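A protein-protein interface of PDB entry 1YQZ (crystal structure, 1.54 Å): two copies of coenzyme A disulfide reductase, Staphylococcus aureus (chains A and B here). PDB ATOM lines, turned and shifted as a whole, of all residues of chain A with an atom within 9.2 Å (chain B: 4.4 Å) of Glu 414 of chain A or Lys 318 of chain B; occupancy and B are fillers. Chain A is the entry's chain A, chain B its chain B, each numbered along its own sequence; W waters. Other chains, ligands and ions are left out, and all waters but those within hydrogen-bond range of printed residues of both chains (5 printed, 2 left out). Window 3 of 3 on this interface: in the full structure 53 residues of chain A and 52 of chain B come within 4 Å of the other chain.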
ATOM      1  N   VAL A 398     -17.741 -15.828 -14.602  1.00  0.00           N
ATOM      2  CA  VAL A 398     -17.239 -15.041 -15.731  1.00  0.00           C
ATOM      3  C   VAL A 398     -16.807 -15.992 -16.862  1.00  0.00           C
ATOM      4  O   VAL A 398     -17.068 -15.732 -18.039  1.00  0.00           O
ATOM      5  CB  VAL A 398     -16.029 -14.150 -15.287  1.00  0.00           C
ATOM      6  CG1 VAL A 398     -15.309 -13.573 -16.484  1.00  0.00           C
ATOM      7  CG2 VAL A 398     -16.513 -13.022 -14.404  1.00  0.00           C
ATOM      8  N   LEU A 407     -15.427 -18.310 -26.351  1.00  0.00           N
ATOM      9  CA  LEU A 407     -14.288 -17.388 -26.281  1.00  0.00           C
ATOM     10  C   LEU A 407     -12.982 -18.191 -26.217  1.00  0.00           C
ATOM     11  O   LEU A 407     -12.972 -19.340 -25.744  1.00  0.00           O
ATOM     12  CB  LEU A 407     -14.373 -16.527 -25.016  1.00  0.00           C
ATOM     13  CG  LEU A 407     -13.430 -15.324 -24.973  1.00  0.00           C
ATOM     14  CD1 LEU A 407     -14.045 -14.225 -25.811  1.00  0.00           C
ATOM     15  CD2 LEU A 407     -13.206 -14.839 -23.546  1.00  0.00           C
ATOM     16  N   THR A 408     -11.890 -17.606 -26.707  1.00  0.00           N
ATOM     17  CA  THR A 408     -10.627 -18.327 -26.639  1.00  0.00           C
ATOM     18  C   THR A 408      -9.847 -17.953 -25.383  1.00  0.00           C
ATOM     19  O   THR A 408     -10.067 -16.906 -24.765  1.00  0.00           O
ATOM     20  CB  THR A 408      -9.715 -18.048 -27.821  1.00  0.00           C
ATOM     21  OG1 THR A 408      -9.285 -16.682 -27.796  1.00  0.00           O
ATOM     22  CG2 THR A 408     -10.441 -18.356 -29.131  1.00  0.00           C
ATOM     23  N   VAL A 409      -8.916 -18.819 -25.026  1.00  0.00           N
ATOM     24  CA  VAL A 409      -8.092 -18.580 -23.838  1.00  0.00           C
ATOM     25  C   VAL A 409      -7.278 -17.299 -23.992  1.00  0.00           C
ATOM     26  O   VAL A 409      -7.092 -16.557 -23.029  1.00  0.00           O
ATOM     27  CB  VAL A 409      -7.173 -19.821 -23.566  1.00  0.00           C
ATOM     28  CG1 VAL A 409      -6.167 -20.020 -24.698  1.00  0.00           C
ATOM     29  CG2 VAL A 409      -6.475 -19.667 -22.199  1.00  0.00           C
ATOM     30  N   ASP A 410      -6.820 -17.014 -25.207  1.00  0.00           N
ATOM     31  CA  ASP A 410      -6.019 -15.826 -25.415  1.00  0.00           C
ATOM     32  C   ASP A 410      -6.785 -14.546 -25.159  1.00  0.00           C
ATOM     33  O   ASP A 410      -6.208 -13.569 -24.675  1.00  0.00           O
ATOM     34  CB  ASP A 410      -5.474 -15.839 -26.831  1.00  0.00           C
ATOM     35  CG  ASP A 410      -4.763 -17.122 -27.122  1.00  0.00           C
ATOM     36  OD1 ASP A 410      -3.613 -17.284 -26.653  1.00  0.00           O
ATOM     37  OD2 ASP A 410      -5.368 -17.982 -27.773  1.00  0.00           O
ATOM     38  N   GLU A 411      -8.073 -14.542 -25.484  1.00  0.00           N
ATOM     39  CA  GLU A 411      -8.885 -13.334 -25.302  1.00  0.00           C
ATOM     40  C   GLU A 411      -9.141 -12.990 -23.843  1.00  0.00           C
ATOM     41  O   GLU A 411      -9.680 -11.918 -23.538  1.00  0.00           O
ATOM     42  CB  GLU A 411     -10.214 -13.475 -26.048  1.00  0.00           C
ATOM     43  CG  GLU A 411     -10.045 -13.463 -27.584  1.00  0.00           C
ATOM     44  CD  GLU A 411     -11.324 -13.853 -28.288  1.00  0.00           C
ATOM     45  OE1 GLU A 411     -11.660 -15.049 -28.311  1.00  0.00           O
ATOM     46  OE2 GLU A 411     -12.014 -12.954 -28.805  1.00  0.00           O
ATOM     47  N   LEU A 412      -8.762 -13.888 -22.930  1.00  0.00           N
ATOM     48  CA  LEU A 412      -8.963 -13.584 -21.532  1.00  0.00           C
ATOM     49  C   LEU A 412      -8.099 -12.386 -21.103  1.00  0.00           C
ATOM     50  O   LEU A 412      -8.386 -11.747 -20.087  1.00  0.00           O
ATOM     51  CB  LEU A 412      -8.668 -14.818 -20.675  1.00  0.00           C
ATOM     52  CG  LEU A 412      -9.636 -15.986 -20.889  1.00  0.00           C
ATOM     53  CD1 LEU A 412      -9.238 -17.140 -19.967  1.00  0.00           C
ATOM     54  CD2 LEU A 412     -11.073 -15.537 -20.550  1.00  0.00           C
ATOM     55  N   THR A 413      -7.046 -12.075 -21.858  1.00  0.00           N
ATOM     56  CA  THR A 413      -6.229 -10.916 -21.505  1.00  0.00           C
ATOM     57  C   THR A 413      -7.039  -9.619 -21.638  1.00  0.00           C
ATOM     58  O   THR A 413      -6.702  -8.601 -21.014  1.00  0.00           O
ATOM     59  CB  THR A 413      -4.998 -10.755 -22.449  1.00  0.00           C
ATOM     60  OG1 THR A 413      -5.460 -10.618 -23.803  1.00  0.00           O
ATOM     61  CG2 THR A 413      -4.095 -11.965 -22.375  1.00  0.00           C
ATOM     62  N   GLU A 414      -8.101  -9.673 -22.441  1.00  0.00           N
ATOM     63  CA  GLU A 414      -8.954  -8.521 -22.735  1.00  0.00           C
ATOM     64  C   GLU A 414     -10.122  -8.312 -21.778  1.00  0.00           C
ATOM     65  O   GLU A 414     -10.822  -7.311 -21.886  1.00  0.00           O
ATOM     66  CB  GLU A 414      -9.534  -8.649 -24.158  1.00  0.00           C
ATOM     67  CG  GLU A 414      -8.476  -8.765 -25.267  1.00  0.00           C
ATOM     68  CD  GLU A 414      -9.075  -9.224 -26.571  1.00  0.00           C
ATOM     69  OE1 GLU A 414     -10.307  -9.171 -26.711  1.00  0.00           O
ATOM     70  OE2 GLU A 414      -8.314  -9.634 -27.467  1.00  0.00           O
ATOM     71  N   PHE A 415     -10.349  -9.269 -20.876  1.00  0.00           N
ATOM     72  CA  PHE A 415     -11.435  -9.163 -19.919  1.00  0.00           C
ATOM     73  C   PHE A 415     -11.180  -7.952 -19.022  1.00  0.00           C
ATOM     74  O   PHE A 415     -10.106  -7.827 -18.432  1.00  0.00           O
ATOM     75  CB  PHE A 415     -11.512 -10.455 -19.090  1.00  0.00           C
ATOM     76  CG  PHE A 415     -12.351 -10.330 -17.853  1.00  0.00           C
ATOM     77  CD1 PHE A 415     -13.698  -9.985 -17.939  1.00  0.00           C
ATOM     78  CD2 PHE A 415     -11.786 -10.545 -16.606  1.00  0.00           C
ATOM     79  CE1 PHE A 415     -14.468  -9.858 -16.767  1.00  0.00           C
ATOM     80  CE2 PHE A 415     -12.538 -10.424 -15.430  1.00  0.00           C
ATOM     81  CZ  PHE A 415     -13.873 -10.078 -15.521  1.00  0.00           C
ATOM     82  N   GLU A 416     -12.178  -7.075 -18.913  1.00  0.00           N
ATOM     83  CA  GLU A 416     -12.042  -5.857 -18.126  1.00  0.00           C
ATOM     84  C   GLU A 416     -12.746  -6.090 -16.796  1.00  0.00           C
ATOM     85  O   GLU A 416     -13.963  -6.028 -16.698  1.00  0.00           O
ATOM     86  CB  GLU A 416     -12.656  -4.681 -18.913  1.00  0.00           C
ATOM     87  CG  GLU A 416     -12.433  -3.338 -18.233  1.00  0.00           C
ATOM     88  CD  GLU A 416     -12.870  -2.155 -19.067  1.00  0.00           C
ATOM     89  OE1 GLU A 416     -13.243  -1.138 -18.450  1.00  0.00           O
ATOM     90  OE2 GLU A 416     -12.822  -2.217 -20.305  1.00  0.00           O
ATOM     91  N   VAL A 417     -11.946  -6.407 -15.789  1.00  0.00           N
ATOM     92  CA  VAL A 417     -12.435  -6.693 -14.441  1.00  0.00           C
ATOM     93  C   VAL A 417     -12.824  -5.410 -13.694  1.00  0.00           C
ATOM     94  O   VAL A 417     -12.378  -4.304 -14.039  1.00  0.00           O
ATOM     95  CB  VAL A 417     -11.306  -7.433 -13.633  1.00  0.00           C
ATOM     96  CG1 VAL A 417     -10.212  -6.419 -13.204  1.00  0.00           C
ATOM     97  CG2 VAL A 417     -11.878  -8.151 -12.410  1.00  0.00           C
ATOM     98  N   PRO A 426      -5.558  -5.444 -10.797  1.00  0.00           N
ATOM     99  CA  PRO A 426      -5.603  -4.717 -12.080  1.00  0.00           C
ATOM    100  C   PRO A 426      -5.489  -5.724 -13.239  1.00  0.00           C
ATOM    101  O   PRO A 426      -6.140  -5.571 -14.272  1.00  0.00           O
ATOM    102  CB  PRO A 426      -4.417  -3.760 -11.972  1.00  0.00           C
ATOM    103  CG  PRO A 426      -4.423  -3.434 -10.475  1.00  0.00           C
ATOM    104  CD  PRO A 426      -4.623  -4.803  -9.855  1.00  0.00           C
ATOM    105  N   ASP A 428      -6.414  -9.255 -13.391  1.00  0.00           N
ATOM    106  CA  ASP A 428      -7.084 -10.264 -12.581  1.00  0.00           C
ATOM    107  C   ASP A 428      -6.579 -11.671 -12.879  1.00  0.00           C
ATOM    108  O   ASP A 428      -5.919 -11.897 -13.884  1.00  0.00           O
ATOM    109  CB  ASP A 428      -8.582 -10.246 -12.866  1.00  0.00           C
ATOM    110  CG  ASP A 428      -9.344 -11.115 -11.905  1.00  0.00           C
ATOM    111  OD1 ASP A 428     -10.133 -11.959 -12.380  1.00  0.00           O
ATOM    112  OD2 ASP A 428      -9.115 -10.951 -10.681  1.00  0.00           O
ATOM    113  N   ILE A 430      -8.157 -14.000 -14.074  1.00  0.00           N
ATOM    114  CA  ILE A 430      -8.637 -14.350 -15.408  1.00  0.00           C
ATOM    115  C   ILE A 430      -7.707 -13.780 -16.495  1.00  0.00           C
ATOM    116  O   ILE A 430      -7.363 -14.463 -17.473  1.00  0.00           O
ATOM    117  CB  ILE A 430     -10.106 -13.876 -15.577  1.00  0.00           C
ATOM    118  CG1 ILE A 430     -11.026 -14.810 -14.772  1.00  0.00           C
ATOM    119  CG2 ILE A 430     -10.528 -13.895 -17.043  1.00  0.00           C
ATOM    120  CD1 ILE A 430     -12.482 -14.409 -14.770  1.00  0.00           C
ATOM    121  N   ASN A 431      -7.278 -12.533 -16.326  1.00  0.00           N
ATOM    122  CA  ASN A 431      -6.355 -11.958 -17.300  1.00  0.00           C
ATOM    123  C   ASN A 431      -5.031 -12.729 -17.316  1.00  0.00           C
ATOM    124  O   ASN A 431      -4.445 -12.953 -18.379  1.00  0.00           O
ATOM    125  CB  ASN A 431      -6.036 -10.496 -16.954  1.00  0.00           C
ATOM    126  CG  ASN A 431      -7.266  -9.586 -16.979  1.00  0.00           C
ATOM    127  OD1 ASN A 431      -7.482  -8.781 -16.040  1.00  0.00           O
ATOM    128  ND2 ASN A 431      -8.054  -9.661 -18.055  1.00  0.00           N
ATOM    129  N   MET A 432      -4.556 -13.111 -16.129  1.00  0.00           N
ATOM    130  CA  MET A 432      -3.291 -13.833 -16.031  1.00  0.00           C
ATOM    131  C   MET A 432      -3.318 -15.178 -16.759  1.00  0.00           C
ATOM    132  O   MET A 432      -2.294 -15.597 -17.310  1.00  0.00           O
ATOM    133  CB  MET A 432      -2.892 -14.026 -14.562  1.00  0.00           C
ATOM    134  CG  MET A 432      -2.572 -12.702 -13.859  1.00  0.00           C
ATOM    135  SD  MET A 432      -1.352 -11.653 -14.747  1.00  0.00           S
ATOM    136  CE  MET A 432      -0.112 -12.878 -15.174  1.00  0.00           C
ATOM    137  N   ILE A 433      -4.463 -15.858 -16.772  1.00  0.00           N
ATOM    138  CA  ILE A 433      -4.566 -17.115 -17.509  1.00  0.00           C
ATOM    139  C   ILE A 433      -4.252 -16.800 -18.987  1.00  0.00           C
ATOM    140  O   ILE A 433      -3.515 -17.522 -19.641  1.00  0.00           O
ATOM    141  CB  ILE A 433      -6.000 -17.722 -17.411  1.00  0.00           C
ATOM    142  CG1 ILE A 433      -6.265 -18.233 -15.988  1.00  0.00           C
ATOM    143  CG2 ILE A 433      -6.165 -18.836 -18.431  1.00  0.00           C
ATOM    144  CD1 ILE A 433      -5.438 -19.495 -15.601  1.00  0.00           C
ATOM    145  N   GLY A 434      -4.817 -15.696 -19.473  1.00  0.00           N
ATOM    146  CA  GLY A 434      -4.623 -15.265 -20.850  1.00  0.00           C
ATOM    147  C   GLY A 434      -3.166 -14.941 -21.138  1.00  0.00           C
ATOM    148  O   GLY A 434      -2.608 -15.375 -22.156  1.00  0.00           O
ATOM    149  N   TYR A 435      -2.535 -14.210 -20.227  1.00  0.00           N
ATOM    150  CA  TYR A 435      -1.125 -13.848 -20.430  1.00  0.00           C
ATOM    151  C   TYR A 435      -0.199 -15.063 -20.361  1.00  0.00           C
ATOM    152  O   TYR A 435       0.839 -15.085 -21.031  1.00  0.00           O
ATOM    153  CB  TYR A 435      -0.682 -12.788 -19.400  1.00  0.00           C
ATOM    154  CG  TYR A 435      -1.270 -11.405 -19.618  1.00  0.00           C
ATOM    155  CD1 TYR A 435      -2.094 -10.817 -18.662  1.00  0.00           C
ATOM    156  CD2 TYR A 435      -1.003 -10.671 -20.788  1.00  0.00           C
ATOM    157  CE1 TYR A 435      -2.639  -9.548 -18.851  1.00  0.00           C
ATOM    158  CE2 TYR A 435      -1.545  -9.401 -20.987  1.00  0.00           C
ATOM    159  CZ  TYR A 435      -2.361  -8.842 -20.018  1.00  0.00           C
ATOM    160  OH  TYR A 435      -2.897  -7.583 -20.191  1.00  0.00           O
ATOM    161  N   LYS A 438       0.581 -18.276 -23.700  1.00  0.00           N
ATOM    162  CA  LYS A 438       1.392 -18.270 -24.913  1.00  0.00           C
ATOM    163  C   LYS A 438       2.725 -18.991 -24.876  1.00  0.00           C
ATOM    164  O   LYS A 438       3.605 -18.593 -25.665  1.00  0.00           O
ATOM    165  CB  LYS A 438       1.599 -16.833 -25.385  1.00  0.00           C
ATOM    166  CG  LYS A 438       0.305 -16.170 -25.798  1.00  0.00           C
ATOM    167  CD  LYS A 438       0.539 -14.914 -26.620  1.00  0.00           C
ATOM    168  CE  LYS A 438      -0.764 -14.488 -27.260  1.00  0.00           C
ATOM    169  NZ  LYS A 438      -1.470 -15.699 -27.777  1.00  0.00           N
ATOM    170  OXT LYS A 438       2.868 -19.969 -24.113  1.00  0.00           O
ATOM    171  N   HIS B 282     -11.717   4.767 -27.099  1.00  0.00           N
ATOM    172  CA  HIS B 282     -13.131   4.612 -27.441  1.00  0.00           C
ATOM    173  C   HIS B 282     -13.711   3.415 -26.700  1.00  0.00           C
ATOM    174  O   HIS B 282     -12.963   2.590 -26.165  1.00  0.00           O
ATOM    175  CB  HIS B 282     -13.262   4.378 -28.947  1.00  0.00           C
ATOM    176  CG  HIS B 282     -12.481   3.195 -29.426  1.00  0.00           C
ATOM    177  ND1 HIS B 282     -12.994   1.913 -29.441  1.00  0.00           N
ATOM    178  CD2 HIS B 282     -11.199   3.093 -29.852  1.00  0.00           C
ATOM    179  CE1 HIS B 282     -12.062   1.075 -29.862  1.00  0.00           C
ATOM    180  NE2 HIS B 282     -10.963   1.764 -30.119  1.00  0.00           N
ATOM    181  N   ARG B 284     -15.565  -0.191 -26.338  1.00  0.00           N
ATOM    182  CA  ARG B 284     -15.457  -1.425 -27.083  1.00  0.00           C
ATOM    183  C   ARG B 284     -16.802  -1.829 -27.691  1.00  0.00           C
ATOM    184  O   ARG B 284     -16.856  -2.368 -28.796  1.00  0.00           O
ATOM    185  CB  ARG B 284     -14.957  -2.553 -26.160  1.00  0.00           C
ATOM    186  CG  ARG B 284     -15.030  -3.922 -26.828  1.00  0.00           C
ATOM    187  CD  ARG B 284     -14.276  -5.009 -26.075  1.00  0.00           C
ATOM    188  NE  ARG B 284     -14.321  -6.246 -26.868  1.00  0.00           N
ATOM    189  CZ  ARG B 284     -13.406  -7.214 -26.830  1.00  0.00           C
ATOM    190  NH1 ARG B 284     -12.352  -7.124 -26.031  1.00  0.00           N
ATOM    191  NH2 ARG B 284     -13.526  -8.271 -27.636  1.00  0.00           N
ATOM    192  N   TRP B 296      -7.077  -0.837 -14.294  1.00  0.00           N
ATOM    193  CA  TRP B 296      -7.110  -1.887 -15.309  1.00  0.00           C
ATOM    194  C   TRP B 296      -6.590  -1.381 -16.644  1.00  0.00           C
ATOM    195  O   TRP B 296      -5.828  -2.075 -17.314  1.00  0.00           O
ATOM    196  CB  TRP B 296      -8.544  -2.415 -15.518  1.00  0.00           C
ATOM    197  CG  TRP B 296      -8.594  -3.498 -16.560  1.00  0.00           C
ATOM    198  CD1 TRP B 296      -8.376  -4.825 -16.368  1.00  0.00           C
ATOM    199  CD2 TRP B 296      -8.807  -3.321 -17.972  1.00  0.00           C
ATOM    200  NE1 TRP B 296      -8.431  -5.493 -17.571  1.00  0.00           N
ATOM    201  CE2 TRP B 296      -8.694  -4.596 -18.571  1.00  0.00           C
ATOM    202  CE3 TRP B 296      -9.089  -2.215 -18.778  1.00  0.00           C
ATOM    203  CZ2 TRP B 296      -8.849  -4.787 -19.964  1.00  0.00           C
ATOM    204  CZ3 TRP B 296      -9.245  -2.397 -20.150  1.00  0.00           C
ATOM    205  CH2 TRP B 296      -9.123  -3.670 -20.727  1.00  0.00           C
ATOM    206  N   ARG B 300      -3.483  -2.648 -18.794  1.00  0.00           N
ATOM    207  CA  ARG B 300      -3.711  -3.285 -20.087  1.00  0.00           C
ATOM    208  C   ARG B 300      -2.925  -2.547 -21.166  1.00  0.00           C
ATOM    209  O   ARG B 300      -2.295  -3.185 -22.035  1.00  0.00           O
ATOM    210  CB  ARG B 300      -5.216  -3.301 -20.418  1.00  0.00           C
ATOM    211  CG  ARG B 300      -5.525  -3.918 -21.805  1.00  0.00           C
ATOM    212  CD  ARG B 300      -5.090  -5.394 -21.875  1.00  0.00           C
ATOM    213  NE  ARG B 300      -5.230  -5.868 -23.242  1.00  0.00           N
ATOM    214  CZ  ARG B 300      -4.455  -6.780 -23.811  1.00  0.00           C
ATOM    215  NH1 ARG B 300      -4.665  -7.120 -25.094  1.00  0.00           N
ATOM    216  NH2 ARG B 300      -3.487  -7.352 -23.118  1.00  0.00           N
ATOM    217  N   GLU B 316      -3.609  -5.338 -30.480  1.00  0.00           N
ATOM    218  CA  GLU B 316      -4.157  -3.985 -30.378  1.00  0.00           C
ATOM    219  C   GLU B 316      -5.333  -3.927 -29.399  1.00  0.00           C
ATOM    220  O   GLU B 316      -6.023  -4.924 -29.170  1.00  0.00           O
ATOM    221  CB  GLU B 316      -4.623  -3.481 -31.764  1.00  0.00           C
ATOM    222  CG  GLU B 316      -3.468  -3.292 -32.761  1.00  0.00           C
ATOM    223  CD  GLU B 316      -3.868  -2.555 -34.043  1.00  0.00           C
ATOM    224  OE1 GLU B 316      -4.831  -1.759 -34.025  1.00  0.00           O
ATOM    225  OE2 GLU B 316      -3.182  -2.756 -35.074  1.00  0.00           O
ATOM    226  N   PHE B 317      -5.551  -2.744 -28.828  1.00  0.00           N
ATOM    227  CA  PHE B 317      -6.634  -2.491 -27.881  1.00  0.00           C
ATOM    228  C   PHE B 317      -7.969  -2.625 -28.621  1.00  0.00           C
ATOM    229  O   PHE B 317      -8.045  -2.326 -29.807  1.00  0.00           O
ATOM    230  CB  PHE B 317      -6.485  -1.053 -27.356  1.00  0.00           C
ATOM    231  CG  PHE B 317      -7.351  -0.717 -26.165  1.00  0.00           C
ATOM    232  CD1 PHE B 317      -7.366  -1.545 -25.040  1.00  0.00           C
ATOM    233  CD2 PHE B 317      -8.084   0.479 -26.142  1.00  0.00           C
ATOM    234  CE1 PHE B 317      -8.095  -1.180 -23.905  1.00  0.00           C
ATOM    235  CE2 PHE B 317      -8.813   0.863 -25.022  1.00  0.00           C
ATOM    236  CZ  PHE B 317      -8.820   0.032 -23.898  1.00  0.00           C
ATOM    237  N   LYS B 318      -9.008  -3.086 -27.940  1.00  0.00           N
ATOM    238  CA  LYS B 318     -10.296  -3.175 -28.608  1.00  0.00           C
ATOM    239  C   LYS B 318     -11.292  -2.198 -27.982  1.00  0.00           C
ATOM    240  O   LYS B 318     -12.489  -2.244 -28.270  1.00  0.00           O
ATOM    241  CB  LYS B 318     -10.811  -4.616 -28.586  1.00  0.00           C
ATOM    242  CG  LYS B 318      -9.945  -5.516 -29.483  1.00  0.00           C
ATOM    243  CD  LYS B 318     -10.314  -6.970 -29.427  1.00  0.00           C
ATOM    244  CE  LYS B 318      -9.374  -7.745 -30.333  1.00  0.00           C
ATOM    245  NZ  LYS B 318      -9.361  -9.199 -30.017  1.00  0.00           N
ATOM    246  N   GLY B 319     -10.785  -1.298 -27.139  1.00  0.00           N
ATOM    247  CA  GLY B 319     -11.668  -0.316 -26.516  1.00  0.00           C
ATOM    248  C   GLY B 319     -12.001  -0.612 -25.065  1.00  0.00           C
ATOM    249  O   GLY B 319     -11.738  -1.715 -24.554  1.00  0.00           O
ATOM    250  N   MET B 404     -18.369  -7.684 -23.781  1.00  0.00           N
ATOM    251  CA  MET B 404     -17.179  -7.923 -24.582  1.00  0.00           C
ATOM    252  C   MET B 404     -17.550  -8.853 -25.752  1.00  0.00           C
ATOM    253  O   MET B 404     -16.961  -8.779 -26.835  1.00  0.00           O
ATOM    254  CB  MET B 404     -16.132  -8.609 -23.692  1.00  0.00           C
ATOM    255  CG  MET B 404     -14.760  -8.753 -24.266  1.00  0.00           C
ATOM    256  SD  MET B 404     -13.772  -9.768 -23.108  1.00  0.00           S
ATOM    257  CE  MET B 404     -13.521 -11.190 -24.151  1.00  0.00           C
HETATM  258  O   HOH W   1      -3.553  -9.952 -25.833  1.00  0.00           O
HETATM  259  O   HOH W   2     -14.595  -7.659 -20.293  1.00  0.00           O
HETATM  260  O   HOH W   3     -11.704 -10.253 -28.574  1.00  0.00           O
HETATM  261  O   HOH W   4     -12.534  -3.595 -22.698  1.00  0.00           O
HETATM  262  O   HOH W   5      -5.214  -5.014 -16.912  1.00  0.00           O
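NH1 of Arg 284 of chain B lies within salt-bridge range of OE1 of Glu 414 of chain A (3.0 Å).
The side-chain amino group (NZ) of Lys 318 of chain B lies within salt-bridge range of the side-chain carboxylate (OE2) of Glu 414 of chain A (2.8 Å).
The backbone carbonyl oxygen (O) of Phe 415 of chain A sits at hydrogen-bond distance from the indole nitrogen (NE1) of Trp 296 of chain B (3.0 Å).
The side-chain hydroxyl (OH) of Tyr 435 of chain A is in hydrogen-bond range of the guanidinium group (NH2) of Arg 300 of chain B, at 3.0 Å.
OG1 of Thr 408 of chain A lies within hydrogen-bond range of OE1 of Glu 411 of chain A, at 2.9 Å.
The backbone carbonyl oxygen of Asp 410 of chain A lies within hydrogen-bond range of the side-chain hydroxyl of Thr 413 of chain A (3.2 Å).
The side-chain amide nitrogen (ND2) of Asn 431 of chain A lies within hydrogen-bond range of the backbone carbonyl oxygen (O) of Leu 412 of chain A (2.9 Å).
ND2 of Asn 431 of chain A sits at hydrogen-bond distance from O of Thr 413 of chain A, at 3.4 Å.
The backbone carbonyl oxygen (O) of Phe 415 of chain A sits at hydrogen-bond distance from the side-chain amide nitrogen (ND2) of Asn 431 of chain A.
N of Asp 428 of chain A lies within hydrogen-bond range of OD1 of Asn 431 of chain A, at 2.9 Å.
Among the printed residues, merely in contact across the chains: Leu 407 of chain A with Met 404 of chain B, Glu 411 of chain A with Met 404 of chain B, Thr 413 of chain A with Arg 300 of chain B, Glu 414 of chain A with Trp 296 of chain B, Phe 415 of chain A with Met 404 of chain B, Glu 416 of chain A with Trp 296 of chain B, Val 417 of chain A with Trp 296 of chain B, Pro 426 of chain A with Trp 296 of chain B and Asn 431 of chain A with Trp 296 of chain B.
Glu 414 of chain A touches just these residues of chain B: Arg 284, Trp 296 and Lys 318.
Of chain A, only Glu 414 (2.8 Å) comes within 4 Å of Lys 318 of chain B.
Of chain A, only Glu 414 comes within 4 Å of Arg 284 of chain B.
No residue of chain A comes within 4 Å of Phe 317 of chain B.
Of the printed residues of chain B, Thr 413 of chain A touches Arg 300.
Of the printed residues of chain B, Glu 416 of chain A touches Trp 296.
Lys 438 of chain A touches none of the printed residues of chain B.
The nearest printed residue of chain B that does not touch Phe 415 of chain A is Arg 284 of chain B (5.9 Å).
Of the 9 printed residues of chain B, 5 touch a printed residue of chain A.
Hydrophobic or aromatic side chains of chain A within 4 Å of the printed part of chain B: Leu 407, Val 417 and Tyr 435.
Among the printed residues, Asp or Glu carboxylates within 4 Å of a Lys or Arg side-chain nitrogen of the other chain: Glu 414 of chain A with Arg 284 of chain B (3.0 Å) and Glu 414 of chain A with Lys 318 of chain B (2.8 Å).
No position is printed for both chains.
Water W3 lies within hydrogen-bond range of the side-chain carboxylate of Glu 414 of chain A, the side-chain carboxylate of Glu 411 of chain A, the guanidinium group of Arg 284 of chain B and the side-chain amino group of Lys 318 of chain B.
Water W4 bridges the backbone carbonyl oxygen of Gly 319 of chain B and the side-chain carboxylate of Glu 416 of chain A.
Water W2 lies within hydrogen-bond range of N of Glu 416 of chain A (2.8 Å) and SD of Met 404 of chain B (3.6 Å).
Water W5 lies within hydrogen-bond range of the backbone carbonyl oxygen (O) of Pro 426 of chain A (2.9 Å), the backbone carbonyl oxygen (O) of Trp 296 of chain B (3.0 Å) and the backbone NH (N) of Arg 300 of chain B (3.5 Å).
Water W1 bridges OG1 of Thr 413 of chain A (2.9 Å) and NH1 of Arg 300 of chain B (3.1 Å).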
